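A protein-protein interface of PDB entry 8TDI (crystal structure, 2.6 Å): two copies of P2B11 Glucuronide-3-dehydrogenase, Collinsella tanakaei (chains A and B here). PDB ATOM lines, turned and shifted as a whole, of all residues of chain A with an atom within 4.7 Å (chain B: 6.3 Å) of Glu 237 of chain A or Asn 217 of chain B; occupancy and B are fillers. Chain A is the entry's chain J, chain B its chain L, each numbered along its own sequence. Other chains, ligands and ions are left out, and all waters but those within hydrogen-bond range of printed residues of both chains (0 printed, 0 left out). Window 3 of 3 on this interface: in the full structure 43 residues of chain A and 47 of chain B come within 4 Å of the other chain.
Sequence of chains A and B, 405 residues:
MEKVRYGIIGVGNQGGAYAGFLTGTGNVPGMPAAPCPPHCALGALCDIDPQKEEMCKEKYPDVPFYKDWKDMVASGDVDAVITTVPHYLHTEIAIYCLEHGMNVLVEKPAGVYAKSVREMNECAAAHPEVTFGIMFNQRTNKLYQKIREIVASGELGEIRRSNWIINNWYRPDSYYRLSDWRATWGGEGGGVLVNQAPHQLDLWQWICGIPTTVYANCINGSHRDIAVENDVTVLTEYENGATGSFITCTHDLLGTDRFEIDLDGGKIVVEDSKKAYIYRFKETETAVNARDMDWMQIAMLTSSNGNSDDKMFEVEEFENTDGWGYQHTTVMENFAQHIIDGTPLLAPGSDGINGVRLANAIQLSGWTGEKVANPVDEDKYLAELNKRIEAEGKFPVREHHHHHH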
ATOM      1  N   PRO A 211      -2.752 -16.431  16.805  1.00  0.00           N
ATOM      2  CA  PRO A 211      -1.950 -15.821  17.857  1.00  0.00           C
ATOM      3  C   PRO A 211      -1.762 -16.724  19.069  1.00  0.00           C
ATOM      4  O   PRO A 211      -2.729 -17.322  19.543  1.00  0.00           O
ATOM      5  CB  PRO A 211      -2.783 -14.570  18.198  1.00  0.00           C
ATOM      6  CG  PRO A 211      -3.618 -14.322  16.983  1.00  0.00           C
ATOM      7  CD  PRO A 211      -3.998 -15.696  16.535  1.00  0.00           C
ATOM      8  N   THR A 212      -0.528 -16.791  19.585  1.00  0.00           N
ATOM      9  CA  THR A 212      -0.279 -17.504  20.832  1.00  0.00           C
ATOM     10  C   THR A 212      -0.931 -16.774  22.007  1.00  0.00           C
ATOM     11  O   THR A 212      -1.504 -17.430  22.878  1.00  0.00           O
ATOM     12  CB  THR A 212       1.222 -17.666  21.045  1.00  0.00           C
ATOM     13  OG1 THR A 212       1.785 -16.373  20.825  1.00  0.00           O
ATOM     14  CG2 THR A 212       1.827 -18.664  20.076  1.00  0.00           C
ATOM     15  N   THR A 213      -0.849 -15.431  22.023  1.00  0.00           N
ATOM     16  CA  THR A 213      -1.355 -14.645  23.143  1.00  0.00           C
ATOM     17  C   THR A 213      -2.169 -13.473  22.604  1.00  0.00           C
ATOM     18  O   THR A 213      -1.823 -12.936  21.558  1.00  0.00           O
ATOM     19  CB  THR A 213      -0.201 -14.125  24.009  1.00  0.00           C
ATOM     20  OG1 THR A 213       0.286 -12.956  23.362  1.00  0.00           O
ATOM     21  CG2 THR A 213       0.923 -15.128  24.187  1.00  0.00           C
ATOM     22  N   LEU A 235      -3.604  -6.540  20.678  1.00  0.00           N
ATOM     23  CA  LEU A 235      -2.235  -6.939  20.388  1.00  0.00           C
ATOM     24  C   LEU A 235      -2.115  -8.448  20.481  1.00  0.00           C
ATOM     25  O   LEU A 235      -2.508  -9.047  21.477  1.00  0.00           O
ATOM     26  CB  LEU A 235      -1.123  -6.423  21.292  1.00  0.00           C
ATOM     27  CG  LEU A 235      -1.099  -4.938  21.623  1.00  0.00           C
ATOM     28  CD1 LEU A 235       0.343  -4.612  22.004  1.00  0.00           C
ATOM     29  CD2 LEU A 235      -1.564  -4.063  20.509  1.00  0.00           C
ATOM     30  N   THR A 236      -1.401  -9.018  19.514  1.00  0.00           N
ATOM     31  CA  THR A 236      -1.189 -10.454  19.461  1.00  0.00           C
ATOM     32  C   THR A 236       0.302 -10.747  19.394  1.00  0.00           C
ATOM     33  O   THR A 236       1.074  -9.895  18.965  1.00  0.00           O
ATOM     34  CB  THR A 236      -1.912 -11.037  18.248  1.00  0.00           C
ATOM     35  OG1 THR A 236      -1.505 -10.240  17.133  1.00  0.00           O
ATOM     36  CG2 THR A 236      -3.421 -11.039  18.432  1.00  0.00           C
ATOM     37  N   GLU A 237       0.657 -11.968  19.828  1.00  0.00           N
ATOM     38  CA  GLU A 237       1.961 -12.572  19.607  1.00  0.00           C
ATOM     39  C   GLU A 237       1.751 -13.912  18.915  1.00  0.00           C
ATOM     40  O   GLU A 237       0.642 -14.446  18.920  1.00  0.00           O
ATOM     41  CB  GLU A 237       2.728 -12.818  20.904  1.00  0.00           C
ATOM     42  CG  GLU A 237       2.819 -11.584  21.796  1.00  0.00           C
ATOM     43  CD  GLU A 237       3.566 -11.859  23.084  1.00  0.00           C
ATOM     44  OE1 GLU A 237       4.725 -11.387  23.184  1.00  0.00           O
ATOM     45  OE2 GLU A 237       2.981 -12.512  23.983  1.00  0.00           O
ATOM     46  N   TYR A 238       2.839 -14.445  18.345  1.00  0.00           N
ATOM     47  CA  TYR A 238       2.783 -15.595  17.457  1.00  0.00           C
ATOM     48  C   TYR A 238       3.948 -16.512  17.812  1.00  0.00           C
ATOM     49  O   TYR A 238       4.967 -16.059  18.321  1.00  0.00           O
ATOM     50  CB  TYR A 238       2.805 -15.085  16.002  1.00  0.00           C
ATOM     51  CG  TYR A 238       1.578 -14.249  15.643  1.00  0.00           C
ATOM     52  CD1 TYR A 238       0.421 -14.847  15.144  1.00  0.00           C
ATOM     53  CD2 TYR A 238       1.556 -12.869  15.865  1.00  0.00           C
ATOM     54  CE1 TYR A 238      -0.704 -14.099  14.868  1.00  0.00           C
ATOM     55  CE2 TYR A 238       0.430 -12.112  15.585  1.00  0.00           C
ATOM     56  CZ  TYR A 238      -0.711 -12.732  15.085  1.00  0.00           C
ATOM     57  OH  TYR A 238      -1.833 -12.000  14.787  1.00  0.00           O
ATOM     58  N   GLU A 239       3.800 -17.815  17.510  1.00  0.00           N
ATOM     59  CA  GLU A 239       4.811 -18.809  17.815  1.00  0.00           C
ATOM     60  C   GLU A 239       6.201 -18.288  17.438  1.00  0.00           C
ATOM     61  O   GLU A 239       7.138 -18.464  18.198  1.00  0.00           O
ATOM     62  CB  GLU A 239       4.478 -20.099  17.050  1.00  0.00           C
ATOM     63  CG  GLU A 239       5.108 -21.375  17.568  1.00  0.00           C
ATOM     64  CD  GLU A 239       4.441 -22.008  18.763  1.00  0.00           C
ATOM     65  OE1 GLU A 239       5.101 -22.962  19.180  1.00  0.00           O
ATOM     66  OE2 GLU A 239       3.345 -21.643  19.248  1.00  0.00           O
ATOM     67  N   ALA A 242       6.627 -12.998  16.117  1.00  0.00           N
ATOM     68  CA  ALA A 242       6.015 -11.851  15.468  1.00  0.00           C
ATOM     69  C   ALA A 242       4.956 -11.251  16.386  1.00  0.00           C
ATOM     70  O   ALA A 242       4.495 -11.905  17.323  1.00  0.00           O
ATOM     71  CB  ALA A 242       5.388 -12.280  14.167  1.00  0.00           C
ATOM     72  N   THR A 243       4.595  -9.996  16.105  1.00  0.00           N
ATOM     73  CA  THR A 243       3.535  -9.304  16.815  1.00  0.00           C
ATOM     74  C   THR A 243       2.433  -8.953  15.825  1.00  0.00           C
ATOM     75  O   THR A 243       2.641  -8.987  14.617  1.00  0.00           O
ATOM     76  CB  THR A 243       4.082  -8.053  17.505  1.00  0.00           C
ATOM     77  OG1 THR A 243       4.634  -7.160  16.545  1.00  0.00           O
ATOM     78  CG2 THR A 243       5.146  -8.430  18.515  1.00  0.00           C
ATOM     79  N   LYS A 371      -3.499  -9.713  29.632  1.00  0.00           N
ATOM     80  CA  LYS A 371      -3.084 -10.565  28.540  1.00  0.00           C
ATOM     81  C   LYS A 371      -3.555 -11.992  28.829  1.00  0.00           C
ATOM     82  O   LYS A 371      -3.559 -12.413  29.980  1.00  0.00           O
ATOM     83  CB  LYS A 371      -1.554 -10.510  28.447  1.00  0.00           C
ATOM     84  CG  LYS A 371      -0.973 -11.224  27.224  1.00  0.00           C
ATOM     85  CD  LYS A 371       0.386 -11.924  27.440  1.00  0.00           C
ATOM     86  CE  LYS A 371       1.706 -11.156  27.342  1.00  0.00           C
ATOM     87  NZ  LYS A 371       2.590 -11.370  26.190  1.00  0.00           N
ATOM     88  N   TYR B 215      -0.474  -0.145  27.998  1.00  0.00           N
ATOM     89  CA  TYR B 215      -0.177  -1.563  27.851  1.00  0.00           C
ATOM     90  C   TYR B 215       0.836  -1.683  26.728  1.00  0.00           C
ATOM     91  O   TYR B 215       0.604  -1.101  25.673  1.00  0.00           O
ATOM     92  CB  TYR B 215      -1.368  -2.475  27.503  1.00  0.00           C
ATOM     93  CG  TYR B 215      -0.934  -3.927  27.350  1.00  0.00           C
ATOM     94  CD1 TYR B 215      -0.611  -4.467  26.113  1.00  0.00           C
ATOM     95  CD2 TYR B 215      -0.801  -4.743  28.461  1.00  0.00           C
ATOM     96  CE1 TYR B 215      -0.202  -5.782  25.980  1.00  0.00           C
ATOM     97  CE2 TYR B 215      -0.348  -6.051  28.352  1.00  0.00           C
ATOM     98  CZ  TYR B 215      -0.055  -6.573  27.106  1.00  0.00           C
ATOM     99  OH  TYR B 215       0.383  -7.861  27.000  1.00  0.00           O
ATOM    100  N   ALA B 216       1.942  -2.409  26.931  1.00  0.00           N
ATOM    101  CA  ALA B 216       2.976  -2.445  25.901  1.00  0.00           C
ATOM    102  C   ALA B 216       3.537  -3.853  25.683  1.00  0.00           C
ATOM    103  O   ALA B 216       3.579  -4.659  26.611  1.00  0.00           O
ATOM    104  CB  ALA B 216       4.072  -1.486  26.235  1.00  0.00           C
ATOM    105  N   ASN B 217       3.960  -4.143  24.443  1.00  0.00           N
ATOM    106  CA  ASN B 217       4.662  -5.380  24.134  1.00  0.00           C
ATOM    107  C   ASN B 217       6.050  -4.997  23.644  1.00  0.00           C
ATOM    108  O   ASN B 217       6.172  -4.451  22.542  1.00  0.00           O
ATOM    109  CB  ASN B 217       3.942  -6.205  23.071  1.00  0.00           C
ATOM    110  CG  ASN B 217       4.476  -7.615  23.015  1.00  0.00           C
ATOM    111  OD1 ASN B 217       3.887  -8.467  23.688  1.00  0.00           O
ATOM    112  ND2 ASN B 217       5.477  -7.922  22.193  1.00  0.00           N
ATOM    113  N   CYS B 218       7.080  -5.206  24.484  1.00  0.00           N
ATOM    114  CA  CYS B 218       8.413  -4.737  24.149  1.00  0.00           C
ATOM    115  C   CYS B 218       9.328  -5.936  23.933  1.00  0.00           C
ATOM    116  O   CYS B 218       9.453  -6.772  24.810  1.00  0.00           O
ATOM    117  CB  CYS B 218       8.942  -3.823  25.241  1.00  0.00           C
ATOM    118  SG  CYS B 218       7.888  -2.381  25.521  1.00  0.00           S
ATOM    119  N   ILE B 219       9.944  -6.027  22.757  1.00  0.00           N
ATOM    120  CA  ILE B 219      10.837  -7.135  22.472  1.00  0.00           C
ATOM    121  C   ILE B 219      12.268  -6.634  22.587  1.00  0.00           C
ATOM    122  O   ILE B 219      12.640  -5.700  21.886  1.00  0.00           O
ATOM    123  CB  ILE B 219      10.579  -7.710  21.072  1.00  0.00           C
ATOM    124  CG1 ILE B 219       9.131  -8.159  20.912  1.00  0.00           C
ATOM    125  CG2 ILE B 219      11.563  -8.842  20.794  1.00  0.00           C
ATOM    126  CD1 ILE B 219       8.766  -8.621  19.515  1.00  0.00           C
ATOM    127  N   ASP B 231      11.583  -3.215  19.438  1.00  0.00           N
ATOM    128  CA  ASP B 231      10.321  -3.442  18.745  1.00  0.00           C
ATOM    129  C   ASP B 231       9.224  -3.302  19.797  1.00  0.00           C
ATOM    130  O   ASP B 231       9.150  -4.108  20.734  1.00  0.00           O
ATOM    131  CB  ASP B 231      10.276  -4.791  18.041  1.00  0.00           C
ATOM    132  CG  ASP B 231       8.990  -5.115  17.289  1.00  0.00           C
ATOM    133  OD1 ASP B 231       7.903  -4.848  17.844  1.00  0.00           O
ATOM    134  OD2 ASP B 231       9.066  -5.666  16.174  1.00  0.00           O
ATOM    135  N   VAL B 232       8.408  -2.251  19.653  1.00  0.00           N
ATOM    136  CA  VAL B 232       7.499  -1.846  20.708  1.00  0.00           C
ATOM    137  C   VAL B 232       6.115  -1.620  20.111  1.00  0.00           C
ATOM    138  O   VAL B 232       5.965  -0.916  19.113  1.00  0.00           O
ATOM    139  CB  VAL B 232       8.016  -0.564  21.390  1.00  0.00           C
ATOM    140  CG1 VAL B 232       7.012  -0.003  22.377  1.00  0.00           C
ATOM    141  CG2 VAL B 232       9.361  -0.786  22.069  1.00  0.00           C
ATOM    142  N   THR B 233       5.099  -2.192  20.763  1.00  0.00           N
ATOM    143  CA  THR B 233       3.725  -1.909  20.405  1.00  0.00           C
ATOM    144  C   THR B 233       3.014  -1.468  21.674  1.00  0.00           C
ATOM    145  O   THR B 233       3.077  -2.190  22.668  1.00  0.00           O
ATOM    146  CB  THR B 233       3.092  -3.185  19.848  1.00  0.00           C
ATOM    147  OG1 THR B 233       3.851  -3.615  18.725  1.00  0.00           O
ATOM    148  CG2 THR B 233       1.666  -2.954  19.394  1.00  0.00           C
ATOM    149  N   VAL B 234       2.325  -0.322  21.631  1.00  0.00           N
ATOM    150  CA  VAL B 234       1.741   0.243  22.838  1.00  0.00           C
ATOM    151  C   VAL B 234       0.255   0.479  22.622  1.00  0.00           C
ATOM    152  O   VAL B 234      -0.088   0.979  21.561  1.00  0.00           O
ATOM    153  CB  VAL B 234       2.423   1.584  23.143  1.00  0.00           C
ATOM    154  CG1 VAL B 234       1.879   2.193  24.437  1.00  0.00           C
ATOM    155  CG2 VAL B 234       3.937   1.461  23.165  1.00  0.00           C
ATOM    156  N   ILE B 362       5.663   2.248  29.540  1.00  0.00           N
ATOM    157  CA  ILE B 362       5.745   1.298  28.449  1.00  0.00           C
ATOM    158  C   ILE B 362       6.697   0.170  28.856  1.00  0.00           C
ATOM    159  O   ILE B 362       6.352  -0.995  28.720  1.00  0.00           O
ATOM    160  CB  ILE B 362       6.177   1.973  27.134  1.00  0.00           C
ATOM    161  CG1 ILE B 362       5.104   2.903  26.597  1.00  0.00           C
ATOM    162  CG2 ILE B 362       6.610   0.952  26.090  1.00  0.00           C
ATOM    163  CD1 ILE B 362       5.603   3.892  25.538  1.00  0.00           C
ATOM    164  N   SER B 365       5.236  -2.050  31.772  1.00  0.00           N
ATOM    165  CA  SER B 365       4.185  -2.888  31.232  1.00  0.00           C
ATOM    166  C   SER B 365       4.820  -4.040  30.473  1.00  0.00           C
ATOM    167  O   SER B 365       4.443  -5.195  30.645  1.00  0.00           O
ATOM    168  CB  SER B 365       3.262  -2.105  30.338  1.00  0.00           C
ATOM    169  OG  SER B 365       2.256  -2.949  29.807  1.00  0.00           O
ATOM    170  N   GLY B 366       5.803  -3.685  29.640  1.00  0.00           N
ATOM    171  CA  GLY B 366       6.551  -4.631  28.831  1.00  0.00           C
ATOM    172  C   GLY B 366       7.212  -5.705  29.683  1.00  0.00           C
ATOM    173  O   GLY B 366       7.163  -6.882  29.350  1.00  0.00           O
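OD1 of Asn 217 of chain B sits close to OE1 of Glu 237 of chain A.
The backbone NH of Ile 219 of chain B is in hydrogen-bond range of the backbone carbonyl oxygen of Asp 231 of chain B, at 2.9 Å.
The side-chain carboxylate (OE2) of Glu 237 of chain A sits at hydrogen-bond distance from the side-chain hydroxyl (OG1) of Thr 213 of chain A (2.8 Å).
The backbone NH (N) of Asn 217 of chain B is in hydrogen-bond range of the backbone carbonyl oxygen (O) of Thr 233 of chain B, 2.8 Å away.
The side-chain carboxylate (OE2) of Glu 237 of chain A is in salt-bridge range of the side-chain amino group (NZ) of Lys 371 of chain A (2.5 Å).
The backbone NH of Thr 212 of chain A sits at hydrogen-bond distance from the backbone carbonyl oxygen of Glu 237 of chain A, at 2.7 Å.
CD1 of Leu 235 of chain A touches CG2 of Thr 233 of chain B, 3.4 Å away.
Thr 243 of chain A touches Asn 217 of chain B.
Thr 243 of chain A touches Ile 219 of chain B.
Lys 371 of chain A touches Tyr 215 of chain B.
Thr 212 of chain A touches none of the printed residues of chain B.
Of chain B, only Asn 217 (3.1 Å) comes within 4 Å of Glu 237 of chain A.
Printed residues of chain B within 4 Å of Lys 371 of chain A: Tyr 215.
Asn 217 of chain B touches just these residues of chain A: Glu 237 and Thr 243.
Of the printed residues of chain A, Ile 219 of chain B touches Thr 243 (3.8 Å).
Asp 231 of chain B touches none of the printed residues of chain A.
The nearest printed residue of chain A that does not touch Tyr 215 of chain B is Leu 235 of chain A (4.2 Å).
Of the 12 printed residues of chain B, 4 touch a printed residue of chain A.
Hydrophobic or aromatic side chains of chain B within 4 Å of the printed part of chain A: Tyr 215 and Ile 219.
Along chain B the printed residues that touch a printed residue of chain A span positions 215 to 233.
Among the printed residues, no Asp or Glu carboxylate lies within 4 Å of a Lys or Arg side-chain nitrogen of the other chain.
No position is printed for both chains.
Of the 5 pairs that touch across the chains among the printed residues, none has its exchanged pair printed and touching as well.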
